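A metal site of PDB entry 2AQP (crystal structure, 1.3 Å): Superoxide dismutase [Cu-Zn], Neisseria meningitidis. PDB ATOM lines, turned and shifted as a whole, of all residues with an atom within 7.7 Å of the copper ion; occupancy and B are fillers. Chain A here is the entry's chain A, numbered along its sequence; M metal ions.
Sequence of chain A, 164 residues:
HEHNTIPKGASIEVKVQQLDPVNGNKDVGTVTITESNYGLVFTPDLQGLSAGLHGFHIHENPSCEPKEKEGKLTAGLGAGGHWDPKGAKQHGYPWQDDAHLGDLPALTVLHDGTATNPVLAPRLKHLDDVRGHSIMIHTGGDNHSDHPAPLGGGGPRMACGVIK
Merely in contact with the copper ion: His 82 and Met 136.
Along chain A the residues within 4 Å of the copper ion span positions 57 to 138.
The nearest printed residue that does not touch the copper ion is Phe 56 (5.2 Å).
The backbone carbonyl oxygen (O) of Gly 55 lies within hydrogen-bond range of the backbone NH (N) of His 138.
N of His 59 sits at hydrogen-bond distance from O of Ser 134, at 2.8 Å.
NE2 of His 57 lies within hydrogen-bond range of OD2 of Asp 142 (2.9 Å).
A ring nitrogen (ND1) of His 138 is in hydrogen-bond range of the backbone carbonyl oxygen (O) of Pro 156 (3.2 Å).
O of Gly 81 sits close to ND1 of His 59 (3.4 Å).
ND1 of His 138 sits at hydrogen-bond distance from O of Gly 155, at 3.0 Å.
ND1 of His 57 lies close to NE2 of His 82, 3.2 Å away.
O of His 57 sits at hydrogen-bond distance from N of Met 136, at 2.8 Å.
The copper ion is bound by ND1 of His 57 (1.9 Å), NE2 of His 59 (1.9 Å) and NE2 of His 138 (2.0 Å).
The copper ion has three donor atoms within binding distance.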
ATOM      1  N   GLY A  55     -24.010 -24.865 -10.252  1.00  0.00           N
ATOM      2  CA  GLY A  55     -24.133 -23.647 -11.013  1.00  0.00           C
ATOM      3  C   GLY A  55     -23.369 -23.740 -12.320  1.00  0.00           C
ATOM      4  O   GLY A  55     -22.287 -24.274 -12.400  1.00  0.00           O
ATOM      5  N   PHE A  56     -23.987 -23.159 -13.353  1.00  0.00           N
ATOM      6  CA  PHE A  56     -23.569 -23.280 -14.727  1.00  0.00           C
ATOM      7  C   PHE A  56     -23.804 -21.968 -15.446  1.00  0.00           C
ATOM      8  O   PHE A  56     -24.965 -21.590 -15.603  1.00  0.00           O
ATOM      9  CB  PHE A  56     -24.368 -24.413 -15.352  1.00  0.00           C
ATOM     10  CG  PHE A  56     -23.960 -24.988 -16.677  1.00  0.00           C
ATOM     11  CD1 PHE A  56     -22.638 -25.272 -16.988  1.00  0.00           C
ATOM     12  CD2 PHE A  56     -24.918 -25.308 -17.632  1.00  0.00           C
ATOM     13  CE1 PHE A  56     -22.310 -25.852 -18.184  1.00  0.00           C
ATOM     14  CE2 PHE A  56     -24.571 -25.899 -18.826  1.00  0.00           C
ATOM     15  CZ  PHE A  56     -23.273 -26.198 -19.096  1.00  0.00           C
ATOM     16  N   HIS A  57     -22.708 -21.289 -15.789  1.00  0.00           N
ATOM     17  CA  HIS A  57     -22.861 -19.944 -16.383  1.00  0.00           C
ATOM     18  C   HIS A  57     -21.793 -19.709 -17.455  1.00  0.00           C
ATOM     19  O   HIS A  57     -20.721 -20.277 -17.435  1.00  0.00           O
ATOM     20  CB  HIS A  57     -22.712 -18.814 -15.368  1.00  0.00           C
ATOM     21  CG  HIS A  57     -23.114 -19.144 -13.970  1.00  0.00           C
ATOM     22  ND1 HIS A  57     -22.216 -19.353 -12.952  1.00  0.00           N
ATOM     23  CD2 HIS A  57     -24.353 -19.376 -13.467  1.00  0.00           C
ATOM     24  CE1 HIS A  57     -22.916 -19.657 -11.859  1.00  0.00           C
ATOM     25  NE2 HIS A  57     -24.223 -19.695 -12.121  1.00  0.00           N
ATOM     26  N   ILE A  58     -22.158 -18.777 -18.367  1.00  0.00           N
ATOM     27  CA  ILE A  58     -21.150 -18.192 -19.234  1.00  0.00           C
ATOM     28  C   ILE A  58     -20.440 -17.067 -18.506  1.00  0.00           C
ATOM     29  O   ILE A  58     -21.107 -16.197 -17.952  1.00  0.00           O
ATOM     30  CB  ILE A  58     -21.816 -17.662 -20.506  1.00  0.00           C
ATOM     31  CG1 ILE A  58     -22.599 -18.741 -21.267  1.00  0.00           C
ATOM     32  CG2 ILE A  58     -20.780 -17.005 -21.387  1.00  0.00           C
ATOM     33  CD1 ILE A  58     -21.702 -19.784 -21.895  1.00  0.00           C
ATOM     34  N   HIS A  59     -19.104 -17.170 -18.531  1.00  0.00           N
ATOM     35  CA  HIS A  59     -18.316 -16.072 -17.942  1.00  0.00           C
ATOM     36  C   HIS A  59     -17.694 -15.229 -19.026  1.00  0.00           C
ATOM     37  O   HIS A  59     -17.625 -15.592 -20.175  1.00  0.00           O
ATOM     38  CB  HIS A  59     -17.252 -16.608 -16.988  1.00  0.00           C
ATOM     39  CG  HIS A  59     -17.821 -17.058 -15.694  1.00  0.00           C
ATOM     40  ND1 HIS A  59     -17.376 -16.604 -14.488  1.00  0.00           N
ATOM     41  CD2 HIS A  59     -18.855 -17.912 -15.370  1.00  0.00           C
ATOM     42  CE1 HIS A  59     -18.066 -17.171 -13.496  1.00  0.00           C
ATOM     43  NE2 HIS A  59     -18.974 -17.974 -13.987  1.00  0.00           N
ATOM     44  N   GLY A  80     -13.020 -14.360 -15.368  1.00  0.00           N
ATOM     45  CA  GLY A  80     -13.709 -13.148 -14.963  1.00  0.00           C
ATOM     46  C   GLY A  80     -15.092 -13.508 -14.449  1.00  0.00           C
ATOM     47  O   GLY A  80     -15.342 -14.644 -14.043  1.00  0.00           O
ATOM     48  N   GLY A  81     -16.003 -12.534 -14.483  1.00  0.00           N
ATOM     49  CA  GLY A  81     -17.306 -12.672 -13.894  1.00  0.00           C
ATOM     50  C   GLY A  81     -18.359 -13.207 -14.843  1.00  0.00           C
ATOM     51  O   GLY A  81     -18.053 -13.597 -15.976  1.00  0.00           O
ATOM     52  N   HIS A  82     -19.598 -13.253 -14.307  1.00  0.00           N
ATOM     53  CA  HIS A  82     -20.705 -13.696 -15.136  1.00  0.00           C
ATOM     54  C   HIS A  82     -20.813 -12.805 -16.363  1.00  0.00           C
ATOM     55  O   HIS A  82     -20.723 -11.590 -16.290  1.00  0.00           O
ATOM     56  CB  HIS A  82     -21.968 -13.693 -14.280  1.00  0.00           C
ATOM     57  CG  HIS A  82     -22.045 -14.793 -13.265  1.00  0.00           C
ATOM     58  ND1 HIS A  82     -23.223 -15.254 -12.735  1.00  0.00           N
ATOM     59  CD2 HIS A  82     -21.061 -15.499 -12.644  1.00  0.00           C
ATOM     60  CE1 HIS A  82     -22.987 -16.212 -11.864  1.00  0.00           C
ATOM     61  NE2 HIS A  82     -21.658 -16.378 -11.785  1.00  0.00           N
ATOM     62  N   TRP A  83     -20.991 -13.405 -17.554  1.00  0.00           N
ATOM     63  CA  TRP A  83     -21.135 -12.589 -18.757  1.00  0.00           C
ATOM     64  C   TRP A  83     -22.389 -11.732 -18.662  1.00  0.00           C
ATOM     65  O   TRP A  83     -23.498 -12.245 -18.446  1.00  0.00           O
ATOM     66  CB  TRP A  83     -21.156 -13.543 -19.944  1.00  0.00           C
ATOM     67  CG  TRP A  83     -21.156 -12.915 -21.308  1.00  0.00           C
ATOM     68  CD1 TRP A  83     -20.412 -11.902 -21.831  1.00  0.00           C
ATOM     69  CD2 TRP A  83     -22.029 -13.327 -22.387  1.00  0.00           C
ATOM     70  NE1 TRP A  83     -20.736 -11.656 -23.133  1.00  0.00           N
ATOM     71  CE2 TRP A  83     -21.736 -12.529 -23.503  1.00  0.00           C
ATOM     72  CE3 TRP A  83     -23.003 -14.305 -22.477  1.00  0.00           C
ATOM     73  CZ2 TRP A  83     -22.412 -12.676 -24.724  1.00  0.00           C
ATOM     74  CZ3 TRP A  83     -23.684 -14.472 -23.663  1.00  0.00           C
ATOM     75  CH2 TRP A  83     -23.379 -13.651 -24.764  1.00  0.00           C
ATOM     76  N   HIS A  91     -27.535 -11.357 -10.595  1.00  0.00           N
ATOM     77  CA  HIS A  91     -27.647 -12.727 -10.972  1.00  0.00           C
ATOM     78  C   HIS A  91     -29.096 -13.166 -10.863  1.00  0.00           C
ATOM     79  O   HIS A  91     -29.809 -12.749  -9.935  1.00  0.00           O
ATOM     80  CB  HIS A  91     -26.725 -13.551 -10.022  1.00  0.00           C
ATOM     81  CG  HIS A  91     -26.717 -14.998 -10.393  1.00  0.00           C
ATOM     82  ND1 HIS A  91     -26.157 -15.489 -11.528  1.00  0.00           N
ATOM     83  CD2 HIS A  91     -27.307 -16.057  -9.760  1.00  0.00           C
ATOM     84  CE1 HIS A  91     -26.371 -16.801 -11.595  1.00  0.00           C
ATOM     85  NE2 HIS A  91     -27.051 -17.184 -10.536  1.00  0.00           N
ATOM     86  N   GLY A 102     -25.384 -14.466 -19.141  1.00  0.00           N
ATOM     87  CA  GLY A 102     -24.726 -15.746 -19.000  1.00  0.00           C
ATOM     88  C   GLY A 102     -25.338 -16.679 -18.005  1.00  0.00           C
ATOM     89  O   GLY A 102     -24.772 -17.778 -17.812  1.00  0.00           O
ATOM     90  N   ASP A 103     -26.457 -16.315 -17.377  1.00  0.00           N
ATOM     91  CA  ASP A 103     -27.063 -17.227 -16.380  1.00  0.00           C
ATOM     92  C   ASP A 103     -27.809 -18.359 -17.047  1.00  0.00           C
ATOM     93  O   ASP A 103     -28.917 -18.182 -17.635  1.00  0.00           O
ATOM     94  CB  ASP A 103     -27.948 -16.399 -15.450  1.00  0.00           C
ATOM     95  CG  ASP A 103     -27.155 -15.432 -14.586  1.00  0.00           C
ATOM     96  OD1 ASP A 103     -25.897 -15.564 -14.524  1.00  0.00           O
ATOM     97  OD2 ASP A 103     -27.814 -14.534 -14.000  1.00  0.00           O
ATOM     98  N   SER A 134     -16.418 -18.079 -21.870  1.00  0.00           N
ATOM     99  CA  SER A 134     -16.122 -19.349 -21.202  1.00  0.00           C
ATOM    100  C   SER A 134     -17.392 -19.894 -20.573  1.00  0.00           C
ATOM    101  O   SER A 134     -18.329 -19.130 -20.322  1.00  0.00           O
ATOM    102  CB  SER A 134     -15.033 -19.176 -20.144  1.00  0.00           C
ATOM    103  OG  SER A 134     -15.324 -18.079 -19.312  1.00  0.00           O
ATOM    104  N   ILE A 135     -17.431 -21.192 -20.379  1.00  0.00           N
ATOM    105  CA  ILE A 135     -18.524 -21.848 -19.676  1.00  0.00           C
ATOM    106  C   ILE A 135     -17.932 -22.431 -18.383  1.00  0.00           C
ATOM    107  O   ILE A 135     -16.886 -23.076 -18.402  1.00  0.00           O
ATOM    108  CB  ILE A 135     -19.239 -22.878 -20.544  1.00  0.00           C
ATOM    109  CG1 ILE A 135     -20.535 -23.377 -19.904  1.00  0.00           C
ATOM    110  CG2 ILE A 135     -18.323 -24.010 -20.930  1.00  0.00           C
ATOM    111  CD1 ILE A 135     -21.509 -23.847 -20.976  1.00  0.00           C
ATOM    112  N   MET A 136     -18.616 -22.149 -17.308  1.00  0.00           N
ATOM    113  CA  MET A 136     -18.162 -22.474 -15.966  1.00  0.00           C
ATOM    114  C   MET A 136     -19.141 -23.396 -15.241  1.00  0.00           C
ATOM    115  O   MET A 136     -20.336 -23.160 -15.273  1.00  0.00           O
ATOM    116  CB  MET A 136     -18.039 -21.201 -15.129  1.00  0.00           C
ATOM    117  CG  MET A 136     -17.197 -21.386 -13.866  1.00  0.00           C
ATOM    118  SD  MET A 136     -15.447 -21.581 -14.249  1.00  0.00           S
ATOM    119  CE  MET A 136     -15.057 -19.982 -14.920  1.00  0.00           C
ATOM    120  N   ILE A 137     -18.579 -24.404 -14.565  1.00  0.00           N
ATOM    121  CA  ILE A 137     -19.331 -25.299 -13.700  1.00  0.00           C
ATOM    122  C   ILE A 137     -18.811 -25.092 -12.271  1.00  0.00           C
ATOM    123  O   ILE A 137     -17.593 -25.219 -12.066  1.00  0.00           O
ATOM    124  CB  ILE A 137     -19.210 -26.765 -14.110  1.00  0.00           C
ATOM    125  CG1 ILE A 137     -19.632 -26.978 -15.566  1.00  0.00           C
ATOM    126  CG2 ILE A 137     -20.017 -27.662 -13.178  1.00  0.00           C
ATOM    127  CD1 ILE A 137     -19.219 -28.317 -16.139  1.00  0.00           C
ATOM    128  N   HIS A 138     -19.681 -24.678 -11.354  1.00  0.00           N
ATOM    129  CA  HIS A 138     -19.284 -24.352 -10.012  1.00  0.00           C
ATOM    130  C   HIS A 138     -19.342 -25.532  -9.068  1.00  0.00           C
ATOM    131  O   HIS A 138     -20.055 -26.498  -9.340  1.00  0.00           O
ATOM    132  CB  HIS A 138     -20.163 -23.217  -9.481  1.00  0.00           C
ATOM    133  CG  HIS A 138     -19.829 -21.910 -10.156  1.00  0.00           C
ATOM    134  ND1 HIS A 138     -18.969 -20.972  -9.638  1.00  0.00           N
ATOM    135  CD2 HIS A 138     -20.223 -21.419 -11.363  1.00  0.00           C
ATOM    136  CE1 HIS A 138     -18.906 -19.943 -10.492  1.00  0.00           C
ATOM    137  NE2 HIS A 138     -19.646 -20.193 -11.545  1.00  0.00           N
ATOM    138  N   ASP A 142     -27.118 -23.235  -7.672  1.00  0.00           N
ATOM    139  CA  ASP A 142     -27.551 -21.941  -8.210  1.00  0.00           C
ATOM    140  C   ASP A 142     -29.013 -21.728  -7.860  1.00  0.00           C
ATOM    141  O   ASP A 142     -29.928 -22.257  -8.487  1.00  0.00           O
ATOM    142  CB  ASP A 142     -27.310 -21.872  -9.700  1.00  0.00           C
ATOM    143  CG  ASP A 142     -27.402 -20.454 -10.274  1.00  0.00           C
ATOM    144  OD1 ASP A 142     -27.894 -19.553  -9.546  1.00  0.00           O
ATOM    145  OD2 ASP A 142     -26.951 -20.295 -11.429  1.00  0.00           O
ATOM    146  N   LEU A 151     -24.266 -14.657  -6.406  1.00  0.00           N
ATOM    147  CA  LEU A 151     -24.104 -15.461  -7.607  1.00  0.00           C
ATOM    148  C   LEU A 151     -24.665 -16.860  -7.450  1.00  0.00           C
ATOM    149  O   LEU A 151     -24.127 -17.859  -7.946  1.00  0.00           O
ATOM    150  CB  LEU A 151     -22.639 -15.463  -8.005  1.00  0.00           C
ATOM    151  CG  LEU A 151     -22.035 -14.080  -8.251  1.00  0.00           C
ATOM    152  CD1 LEU A 151     -20.534 -14.160  -8.499  1.00  0.00           C
ATOM    153  CD2 LEU A 151     -22.709 -13.380  -9.402  1.00  0.00           C
ATOM    154  N   GLY A 154     -22.967 -20.351  -6.110  1.00  0.00           N
ATOM    155  CA  GLY A 154     -22.089 -21.180  -6.892  1.00  0.00           C
ATOM    156  C   GLY A 154     -20.720 -21.393  -6.273  1.00  0.00           C
ATOM    157  O   GLY A 154     -20.135 -22.474  -6.340  1.00  0.00           O
ATOM    158  N   GLY A 155     -20.190 -20.332  -5.669  1.00  0.00           N
ATOM    159  CA  GLY A 155     -18.913 -20.462  -5.006  1.00  0.00           C
ATOM    160  C   GLY A 155     -17.778 -20.793  -5.957  1.00  0.00           C
ATOM    161  O   GLY A 155     -17.767 -20.214  -7.036  1.00  0.00           O
ATOM    162  N   PRO A 156     -16.832 -21.615  -5.548  1.00  0.00           N
ATOM    163  CA  PRO A 156     -15.677 -21.900  -6.346  1.00  0.00           C
ATOM    164  C   PRO A 156     -15.951 -22.513  -7.720  1.00  0.00           C
ATOM    165  O   PRO A 156     -17.059 -23.001  -8.002  1.00  0.00           O
ATOM    166  CB  PRO A 156     -14.894 -22.927  -5.474  1.00  0.00           C
ATOM    167  CG  PRO A 156     -15.287 -22.611  -4.101  1.00  0.00           C
ATOM    168  CD  PRO A 156     -16.750 -22.256  -4.227  1.00  0.00           C
ATOM    169  N   ARG A 157     -14.949 -22.468  -8.549  1.00  0.00           N
ATOM    170  CA  ARG A 157     -15.006 -22.919  -9.943  1.00  0.00           C
ATOM    171  C   ARG A 157     -14.400 -24.320 -10.092  1.00  0.00           C
ATOM    172  O   ARG A 157     -13.226 -24.488  -9.849  1.00  0.00           O
ATOM    173  CB  ARG A 157     -14.317 -21.856 -10.819  1.00  0.00           C
ATOM    174  CG  ARG A 157     -14.947 -20.494 -10.671  1.00  0.00           C
ATOM    175  CD  ARG A 157     -14.145 -19.366 -11.255  1.00  0.00           C
ATOM    176  NE  ARG A 157     -14.841 -18.121 -10.937  1.00  0.00           N
ATOM    177  CZ  ARG A 157     -14.807 -16.991 -11.605  1.00  0.00           C
ATOM    178  NH1 ARG A 157     -14.080 -16.861 -12.689  1.00  0.00           N
ATOM    179  NH2 ARG A 157     -15.516 -15.964 -11.158  1.00  0.00           N
HETATM  180 CU    CU M   1     -20.318 -18.982 -13.025  1.00  0.00          CU
HETATM  181 ZN    ZN M   2     -25.115 -14.614 -13.067  1.00  0.00          ZN
